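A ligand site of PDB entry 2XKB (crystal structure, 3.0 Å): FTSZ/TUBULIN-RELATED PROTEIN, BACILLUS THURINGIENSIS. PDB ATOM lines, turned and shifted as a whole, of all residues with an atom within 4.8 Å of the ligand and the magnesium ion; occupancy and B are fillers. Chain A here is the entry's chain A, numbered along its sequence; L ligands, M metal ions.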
ATOM      1  N   GLY A  31     -12.743  18.376  17.161  1.00  0.00           N
ATOM      2  CA  GLY A  31     -11.381  18.922  17.118  1.00  0.00           C
ATOM      3  C   GLY A  31     -11.174  19.967  18.196  1.00  0.00           C
ATOM      4  O   GLY A  31     -12.145  20.471  18.760  1.00  0.00           O
ATOM      5  N   GLN A  32      -9.935  20.308  18.467  1.00  0.00           N
ATOM      6  CA  GLN A  32      -9.664  21.098  19.646  1.00  0.00           C
ATOM      7  C   GLN A  32     -10.379  22.424  19.664  1.00  0.00           C
ATOM      8  O   GLN A  32     -10.948  22.785  20.672  1.00  0.00           O
ATOM      9  CB  GLN A  32      -8.181  21.306  19.860  1.00  0.00           C
ATOM     10  CG  GLN A  32      -7.918  21.841  21.239  1.00  0.00           C
ATOM     11  CD  GLN A  32      -6.552  21.474  21.729  1.00  0.00           C
ATOM     12  OE1 GLN A  32      -6.263  21.619  22.918  1.00  0.00           O
ATOM     13  NE2 GLN A  32      -5.689  20.965  20.837  1.00  0.00           N
ATOM     14  N   LYS A  33     -10.357  23.146  18.566  1.00  0.00           N
ATOM     15  CA  LYS A  33     -11.121  24.372  18.455  1.00  0.00           C
ATOM     16  C   LYS A  33     -12.590  24.073  18.781  1.00  0.00           C
ATOM     17  O   LYS A  33     -13.200  24.751  19.609  1.00  0.00           O
ATOM     18  CB  LYS A  33     -10.990  24.970  17.058  1.00  0.00           C
ATOM     19  CG  LYS A  33     -11.639  26.340  16.867  1.00  0.00           C
ATOM     20  CD  LYS A  33     -13.104  26.274  16.421  1.00  0.00           C
ATOM     21  CE  LYS A  33     -13.596  27.623  15.992  1.00  0.00           C
ATOM     22  NZ  LYS A  33     -14.964  27.575  15.419  1.00  0.00           N
ATOM     23  N   LYS A  36     -13.365  23.290  22.453  1.00  0.00           N
ATOM     24  CA  LYS A  36     -13.245  24.485  23.265  1.00  0.00           C
ATOM     25  C   LYS A  36     -14.456  25.411  23.171  1.00  0.00           C
ATOM     26  O   LYS A  36     -14.877  25.977  24.182  1.00  0.00           O
ATOM     27  CB  LYS A  36     -11.960  25.231  22.909  1.00  0.00           C
ATOM     28  CG  LYS A  36     -10.740  24.562  23.493  1.00  0.00           C
ATOM     29  CD  LYS A  36      -9.523  25.425  23.437  1.00  0.00           C
ATOM     30  CE  LYS A  36      -8.871  25.337  22.094  1.00  0.00           C
ATOM     31  NZ  LYS A  36      -7.494  25.897  22.164  1.00  0.00           N
ATOM     32  N   ASN A  59     -13.563  13.922  19.384  1.00  0.00           N
ATOM     33  CA  ASN A  59     -12.167  13.984  18.965  1.00  0.00           C
ATOM     34  C   ASN A  59     -11.537  12.618  18.807  1.00  0.00           C
ATOM     35  O   ASN A  59     -12.115  11.577  19.198  1.00  0.00           O
ATOM     36  CB  ASN A  59     -11.340  14.795  19.958  1.00  0.00           C
ATOM     37  CG  ASN A  59     -10.199  15.540  19.297  1.00  0.00           C
ATOM     38  OD1 ASN A  59      -9.454  14.986  18.491  1.00  0.00           O
ATOM     39  ND2 ASN A  59     -10.051  16.816  19.637  1.00  0.00           N
ATOM     40  N   ALA A  61      -7.810  12.663  19.247  1.00  0.00           N
ATOM     41  CA  ALA A  61      -6.862  12.847  20.330  1.00  0.00           C
ATOM     42  C   ALA A  61      -7.643  13.059  21.609  1.00  0.00           C
ATOM     43  O   ALA A  61      -8.575  13.876  21.642  1.00  0.00           O
ATOM     44  CB  ALA A  61      -5.995  14.024  20.070  1.00  0.00           C
ATOM     45  N   ASP A  64      -6.945  16.545  23.520  1.00  0.00           N
ATOM     46  CA  ASP A  64      -7.656  17.757  23.136  1.00  0.00           C
ATOM     47  C   ASP A  64      -8.945  17.815  23.944  1.00  0.00           C
ATOM     48  O   ASP A  64      -9.872  18.543  23.573  1.00  0.00           O
ATOM     49  CB  ASP A  64      -8.017  17.778  21.623  1.00  0.00           C
ATOM     50  CG  ASP A  64      -6.802  17.762  20.680  1.00  0.00           C
ATOM     51  OD1 ASP A  64      -5.617  17.672  21.105  1.00  0.00           O
ATOM     52  OD2 ASP A  64      -7.041  17.841  19.455  1.00  0.00           O
ATOM     53  N   GLY A 136     -12.625  24.018  13.790  1.00  0.00           N
ATOM     54  CA  GLY A 136     -11.598  24.944  13.358  1.00  0.00           C
ATOM     55  C   GLY A 136     -11.136  24.342  12.060  1.00  0.00           C
ATOM     56  O   GLY A 136     -10.290  23.439  12.051  1.00  0.00           O
ATOM     57  N   ALA A 137     -11.748  24.776  10.960  1.00  0.00           N
ATOM     58  CA  ALA A 137     -11.342  24.297   9.648  1.00  0.00           C
ATOM     59  C   ALA A 137      -9.848  24.572   9.469  1.00  0.00           C
ATOM     60  O   ALA A 137      -9.345  25.660   9.817  1.00  0.00           O
ATOM     61  CB  ALA A 137     -12.150  24.937   8.551  1.00  0.00           C
ATOM     62  N   GLY A 139      -7.624  21.978  10.614  1.00  0.00           N
ATOM     63  CA  GLY A 139      -7.003  20.907  11.402  1.00  0.00           C
ATOM     64  C   GLY A 139      -7.165  19.598  10.687  1.00  0.00           C
ATOM     65  O   GLY A 139      -7.544  19.568   9.525  1.00  0.00           O
ATOM     66  N   GLY A 140      -6.905  18.500  11.388  1.00  0.00           N
ATOM     67  CA  GLY A 140      -7.113  17.165  10.817  1.00  0.00           C
ATOM     68  C   GLY A 140      -8.400  16.508  11.301  1.00  0.00           C
ATOM     69  O   GLY A 140      -9.196  15.988  10.511  1.00  0.00           O
ATOM     70  N   VAL A 141      -8.570  16.544  12.617  1.00  0.00           N
ATOM     71  CA  VAL A 141      -9.782  16.064  13.273  1.00  0.00           C
ATOM     72  C   VAL A 141     -10.942  16.993  12.900  1.00  0.00           C
ATOM     73  O   VAL A 141     -12.014  16.544  12.486  1.00  0.00           O
ATOM     74  CB  VAL A 141      -9.600  16.043  14.823  1.00  0.00           C
ATOM     75  CG1 VAL A 141     -10.650  15.167  15.463  1.00  0.00           C
ATOM     76  CG2 VAL A 141      -8.204  15.541  15.221  1.00  0.00           C
ATOM     77  N   GLY A 142     -10.695  18.288  13.022  1.00  0.00           N
ATOM     78  CA  GLY A 142     -11.745  19.276  12.842  1.00  0.00           C
ATOM     79  C   GLY A 142     -12.288  19.245  11.434  1.00  0.00           C
ATOM     80  O   GLY A 142     -13.429  18.863  11.217  1.00  0.00           O
ATOM     81  N   SER A 167     -14.087  28.056  11.875  1.00  0.00           N
ATOM     82  CA  SER A 167     -13.009  28.995  11.971  1.00  0.00           C
ATOM     83  C   SER A 167     -12.110  28.842  10.750  1.00  0.00           C
ATOM     84  O   SER A 167     -11.873  27.728  10.277  1.00  0.00           O
ATOM     85  CB  SER A 167     -12.207  28.669  13.221  1.00  0.00           C
ATOM     86  OG  SER A 167     -11.133  29.560  13.399  1.00  0.00           O
ATOM     87  N   PRO A 169      -8.237  29.393   9.220  1.00  0.00           N
ATOM     88  CA  PRO A 169      -6.875  29.375   9.741  1.00  0.00           C
ATOM     89  C   PRO A 169      -6.101  30.659   9.503  1.00  0.00           C
ATOM     90  O   PRO A 169      -6.372  31.365   8.541  1.00  0.00           O
ATOM     91  CB  PRO A 169      -6.228  28.223   8.980  1.00  0.00           C
ATOM     92  CG  PRO A 169      -6.996  28.111   7.719  1.00  0.00           C
ATOM     93  CD  PRO A 169      -8.400  28.439   8.104  1.00  0.00           C
ATOM     94  N   GLU A 175      -2.833  24.016   6.668  1.00  0.00           N
ATOM     95  CA  GLU A 175      -4.118  24.357   7.251  1.00  0.00           C
ATOM     96  C   GLU A 175      -4.966  25.083   6.210  1.00  0.00           C
ATOM     97  O   GLU A 175      -6.152  24.809   6.079  1.00  0.00           O
ATOM     98  CB  GLU A 175      -3.938  25.209   8.503  1.00  0.00           C
ATOM     99  CG  GLU A 175      -3.440  24.434   9.715  1.00  0.00           C
ATOM    100  CD  GLU A 175      -3.209  25.310  10.950  1.00  0.00           C
ATOM    101  OE1 GLU A 175      -2.559  24.825  11.893  1.00  0.00           O
ATOM    102  OE2 GLU A 175      -3.675  26.467  10.989  1.00  0.00           O
ATOM    103  N   ASN A 213      -9.720  33.838  11.609  1.00  0.00           N
ATOM    104  CA  ASN A 213      -8.687  33.935  12.641  1.00  0.00           C
ATOM    105  C   ASN A 213      -7.769  35.126  12.486  1.00  0.00           C
ATOM    106  O   ASN A 213      -7.334  35.714  13.492  1.00  0.00           O
ATOM    107  CB  ASN A 213      -7.810  32.685  12.681  1.00  0.00           C
ATOM    108  CG  ASN A 213      -8.406  31.575  13.517  1.00  0.00           C
ATOM    109  OD1 ASN A 213      -9.469  31.724  14.138  1.00  0.00           O
ATOM    110  ND2 ASN A 213      -7.716  30.444  13.550  1.00  0.00           N
ATOM    111  N   MET A 216      -9.851  38.085  13.499  1.00  0.00           N
ATOM    112  CA  MET A 216     -10.122  38.050  14.931  1.00  0.00           C
ATOM    113  C   MET A 216      -8.924  38.457  15.777  1.00  0.00           C
ATOM    114  O   MET A 216      -9.061  39.263  16.708  1.00  0.00           O
ATOM    115  CB  MET A 216     -10.648  36.672  15.337  1.00  0.00           C
ATOM    116  CG  MET A 216     -12.034  36.388  14.772  1.00  0.00           C
ATOM    117  SD  MET A 216     -12.917  35.049  15.589  1.00  0.00           S
ATOM    118  CE  MET A 216     -11.922  33.630  15.165  1.00  0.00           C
ATOM    119  N   TRP A 236      -5.447  34.900  22.853  1.00  0.00           N
ATOM    120  CA  TRP A 236      -6.274  35.403  21.748  1.00  0.00           C
ATOM    121  C   TRP A 236      -7.483  34.528  21.355  1.00  0.00           C
ATOM    122  O   TRP A 236      -8.563  35.057  21.039  1.00  0.00           O
ATOM    123  CB  TRP A 236      -5.448  35.884  20.537  1.00  0.00           C
ATOM    124  CG  TRP A 236      -5.008  34.846  19.564  1.00  0.00           C
ATOM    125  CD1 TRP A 236      -3.762  34.307  19.467  1.00  0.00           C
ATOM    126  CD2 TRP A 236      -5.793  34.243  18.525  1.00  0.00           C
ATOM    127  NE1 TRP A 236      -3.717  33.394  18.433  1.00  0.00           N
ATOM    128  CE2 TRP A 236      -4.954  33.330  17.844  1.00  0.00           C
ATOM    129  CE3 TRP A 236      -7.123  34.362  18.104  1.00  0.00           C
ATOM    130  CZ2 TRP A 236      -5.400  32.561  16.770  1.00  0.00           C
ATOM    131  CZ3 TRP A 236      -7.569  33.594  17.030  1.00  0.00           C
ATOM    132  CH2 TRP A 236      -6.709  32.704  16.378  1.00  0.00           C
ATOM    133  N   LYS A 237      -7.327  33.207  21.395  1.00  0.00           N
ATOM    134  CA  LYS A 237      -8.422  32.278  21.045  1.00  0.00           C
ATOM    135  C   LYS A 237      -9.501  32.202  22.137  1.00  0.00           C
ATOM    136  O   LYS A 237     -10.695  32.099  21.834  1.00  0.00           O
ATOM    137  CB  LYS A 237      -7.904  30.862  20.744  1.00  0.00           C
ATOM    138  CG  LYS A 237      -6.885  30.783  19.621  1.00  0.00           C
ATOM    139  CD  LYS A 237      -6.081  29.500  19.711  1.00  0.00           C
ATOM    140  CE  LYS A 237      -4.693  29.700  19.153  1.00  0.00           C
ATOM    141  NZ  LYS A 237      -3.676  29.021  20.001  1.00  0.00           N
ATOM    142  N   ALA A 240     -11.411  35.264  21.537  1.00  0.00           N
ATOM    143  CA  ALA A 240     -12.229  35.096  20.325  1.00  0.00           C
ATOM    144  C   ALA A 240     -13.415  34.177  20.599  1.00  0.00           C
ATOM    145  O   ALA A 240     -14.558  34.515  20.294  1.00  0.00           O
ATOM    146  CB  ALA A 240     -11.402  34.562  19.169  1.00  0.00           C
ATOM    147  N   ASN A 241     -13.113  33.024  21.188  1.00  0.00           N
ATOM    148  CA  ASN A 241     -14.150  32.064  21.557  1.00  0.00           C
ATOM    149  C   ASN A 241     -15.251  32.696  22.412  1.00  0.00           C
ATOM    150  O   ASN A 241     -16.426  32.488  22.141  1.00  0.00           O
ATOM    151  CB  ASN A 241     -13.544  30.870  22.289  1.00  0.00           C
ATOM    152  CG  ASN A 241     -12.687  30.022  21.401  1.00  0.00           C
ATOM    153  OD1 ASN A 241     -12.691  30.191  20.175  1.00  0.00           O
ATOM    154  ND2 ASN A 241     -11.923  29.119  22.004  1.00  0.00           N
HETATM  155  P1  LIG L   1      -7.555  19.706  15.279  1.00  0.00           P
HETATM  156  O1  LIG L   1      -7.732  18.611  16.323  1.00  0.00           O
HETATM  157  O2  LIG L   1      -6.861  19.109  14.080  1.00  0.00           O
HETATM  158  O3  LIG L   1      -8.854  20.306  14.831  1.00  0.00           O
HETATM  159  O4  LIG L   1      -6.625  20.831  15.960  1.00  0.00           O
HETATM  160  P2  LIG L   1      -7.134  22.346  16.088  1.00  0.00           P
HETATM  161  O5  LIG L   1      -6.162  23.138  16.955  1.00  0.00           O
HETATM  162  O6  LIG L   1      -8.533  22.322  16.614  1.00  0.00           O
HETATM  163  O7  LIG L   1      -7.179  22.912  14.590  1.00  0.00           O
HETATM  164  C1  LIG L   1      -8.184  23.852  14.223  1.00  0.00           C
HETATM  165  C2  LIG L   1      -7.649  25.211  13.755  1.00  0.00           C
HETATM  166  O8  LIG L   1      -8.269  26.266  14.509  1.00  0.00           O
HETATM  167  C3  LIG L   1      -6.158  25.438  13.911  1.00  0.00           C
HETATM  168  O9  LIG L   1      -5.729  26.123  12.719  1.00  0.00           O
HETATM  169  C4  LIG L   1      -6.027  26.319  15.134  1.00  0.00           C
HETATM  170  O10 LIG L   1      -4.980  27.265  14.969  1.00  0.00           O
HETATM  171  C5  LIG L   1      -7.331  27.064  15.227  1.00  0.00           C
HETATM  172  N1  LIG L   1      -7.838  27.155  16.615  1.00  0.00           N
HETATM  173  C6  LIG L   1      -7.485  26.366  17.651  1.00  0.00           C
HETATM  174  N2  LIG L   1      -8.162  26.690  18.787  1.00  0.00           N
HETATM  175  C7  LIG L   1      -8.974  27.715  18.459  1.00  0.00           C
HETATM  176  C8  LIG L   1      -9.963  28.536  19.183  1.00  0.00           C
HETATM  177  O11 LIG L   1     -10.154  28.322  20.386  1.00  0.00           O
HETATM  178  N3  LIG L   1     -10.604  29.501  18.525  1.00  0.00           N
HETATM  179  C9  LIG L   1     -10.393  29.748  17.228  1.00  0.00           C
HETATM  180  N4  LIG L   1     -11.108  30.745  16.660  1.00  0.00           N
HETATM  181  N5  LIG L   1      -9.501  29.038  16.481  1.00  0.00           N
HETATM  182  C10 LIG L   1      -8.781  28.024  17.032  1.00  0.00           C
HETATM  183 MG    MG M   1      -5.653  18.150  17.726  1.00  0.00          MG
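N of Lys 33 sits at hydrogen-bond distance from O6 of the ligand (2.8 Å). N of Gly 142 is in hydrogen-bond range of O3 of the ligand (3.3 Å). N of Gly 140 sits at hydrogen-bond distance from O2 of the ligand. The backbone NH (N) of Val 141 is in hydrogen-bond range of an oxygen (O2) of the ligand (3.4 Å). A nitrogen (N4) of the ligand sits at hydrogen-bond distance from the side-chain amide oxygen of Asn 213, at 3.2 Å. The backbone NH (N) of Gln 32 is in hydrogen-bond range of an oxygen (O6) of the ligand, 3.1 Å away. The side-chain carboxylate (OE2) of Glu 175 lies within hydrogen-bond range of an oxygen (O9) of the ligand (2.7 Å). The side-chain hydroxyl (OG) of Ser 167 lies within hydrogen-bond range of a nitrogen (N4) of the ligand (3.5 Å). ND2 of Asn 241 sits at hydrogen-bond distance from O11 of the ligand (2.5 Å).
The side-chain amide nitrogen (ND2) of Asn 59 sits close to the side-chain carboxylate (OD2) of Asp 64, 3.2 Å away. OG of Ser 167 sits at hydrogen-bond distance from OD1 of Asn 213. N of Ala 137 lies within hydrogen-bond range of O of Ser 167 (3.0 Å). The side-chain amide oxygen of Asn 241 lies close to the backbone carbonyl oxygen of Lys 237, at 3.2 Å. The side-chain carboxylate (OD1) of Asp 64 lies within hydrogen-bond range of the side-chain amide nitrogen (NE2) of Gln 32 (3.3 Å).
Residues that only touch the ligand: Gly 31, Lys 36, Gly 136, Gly 139, Met 216 and Lys 237. Hydrophobic or aromatic side chains that line the ligand: Val 141 and Met 216.
The magnesium ion is bound by the side-chain carboxylate (OD2) of Asp 64 (2.2 Å) and an oxygen (O1) of the ligand (2.6 Å).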
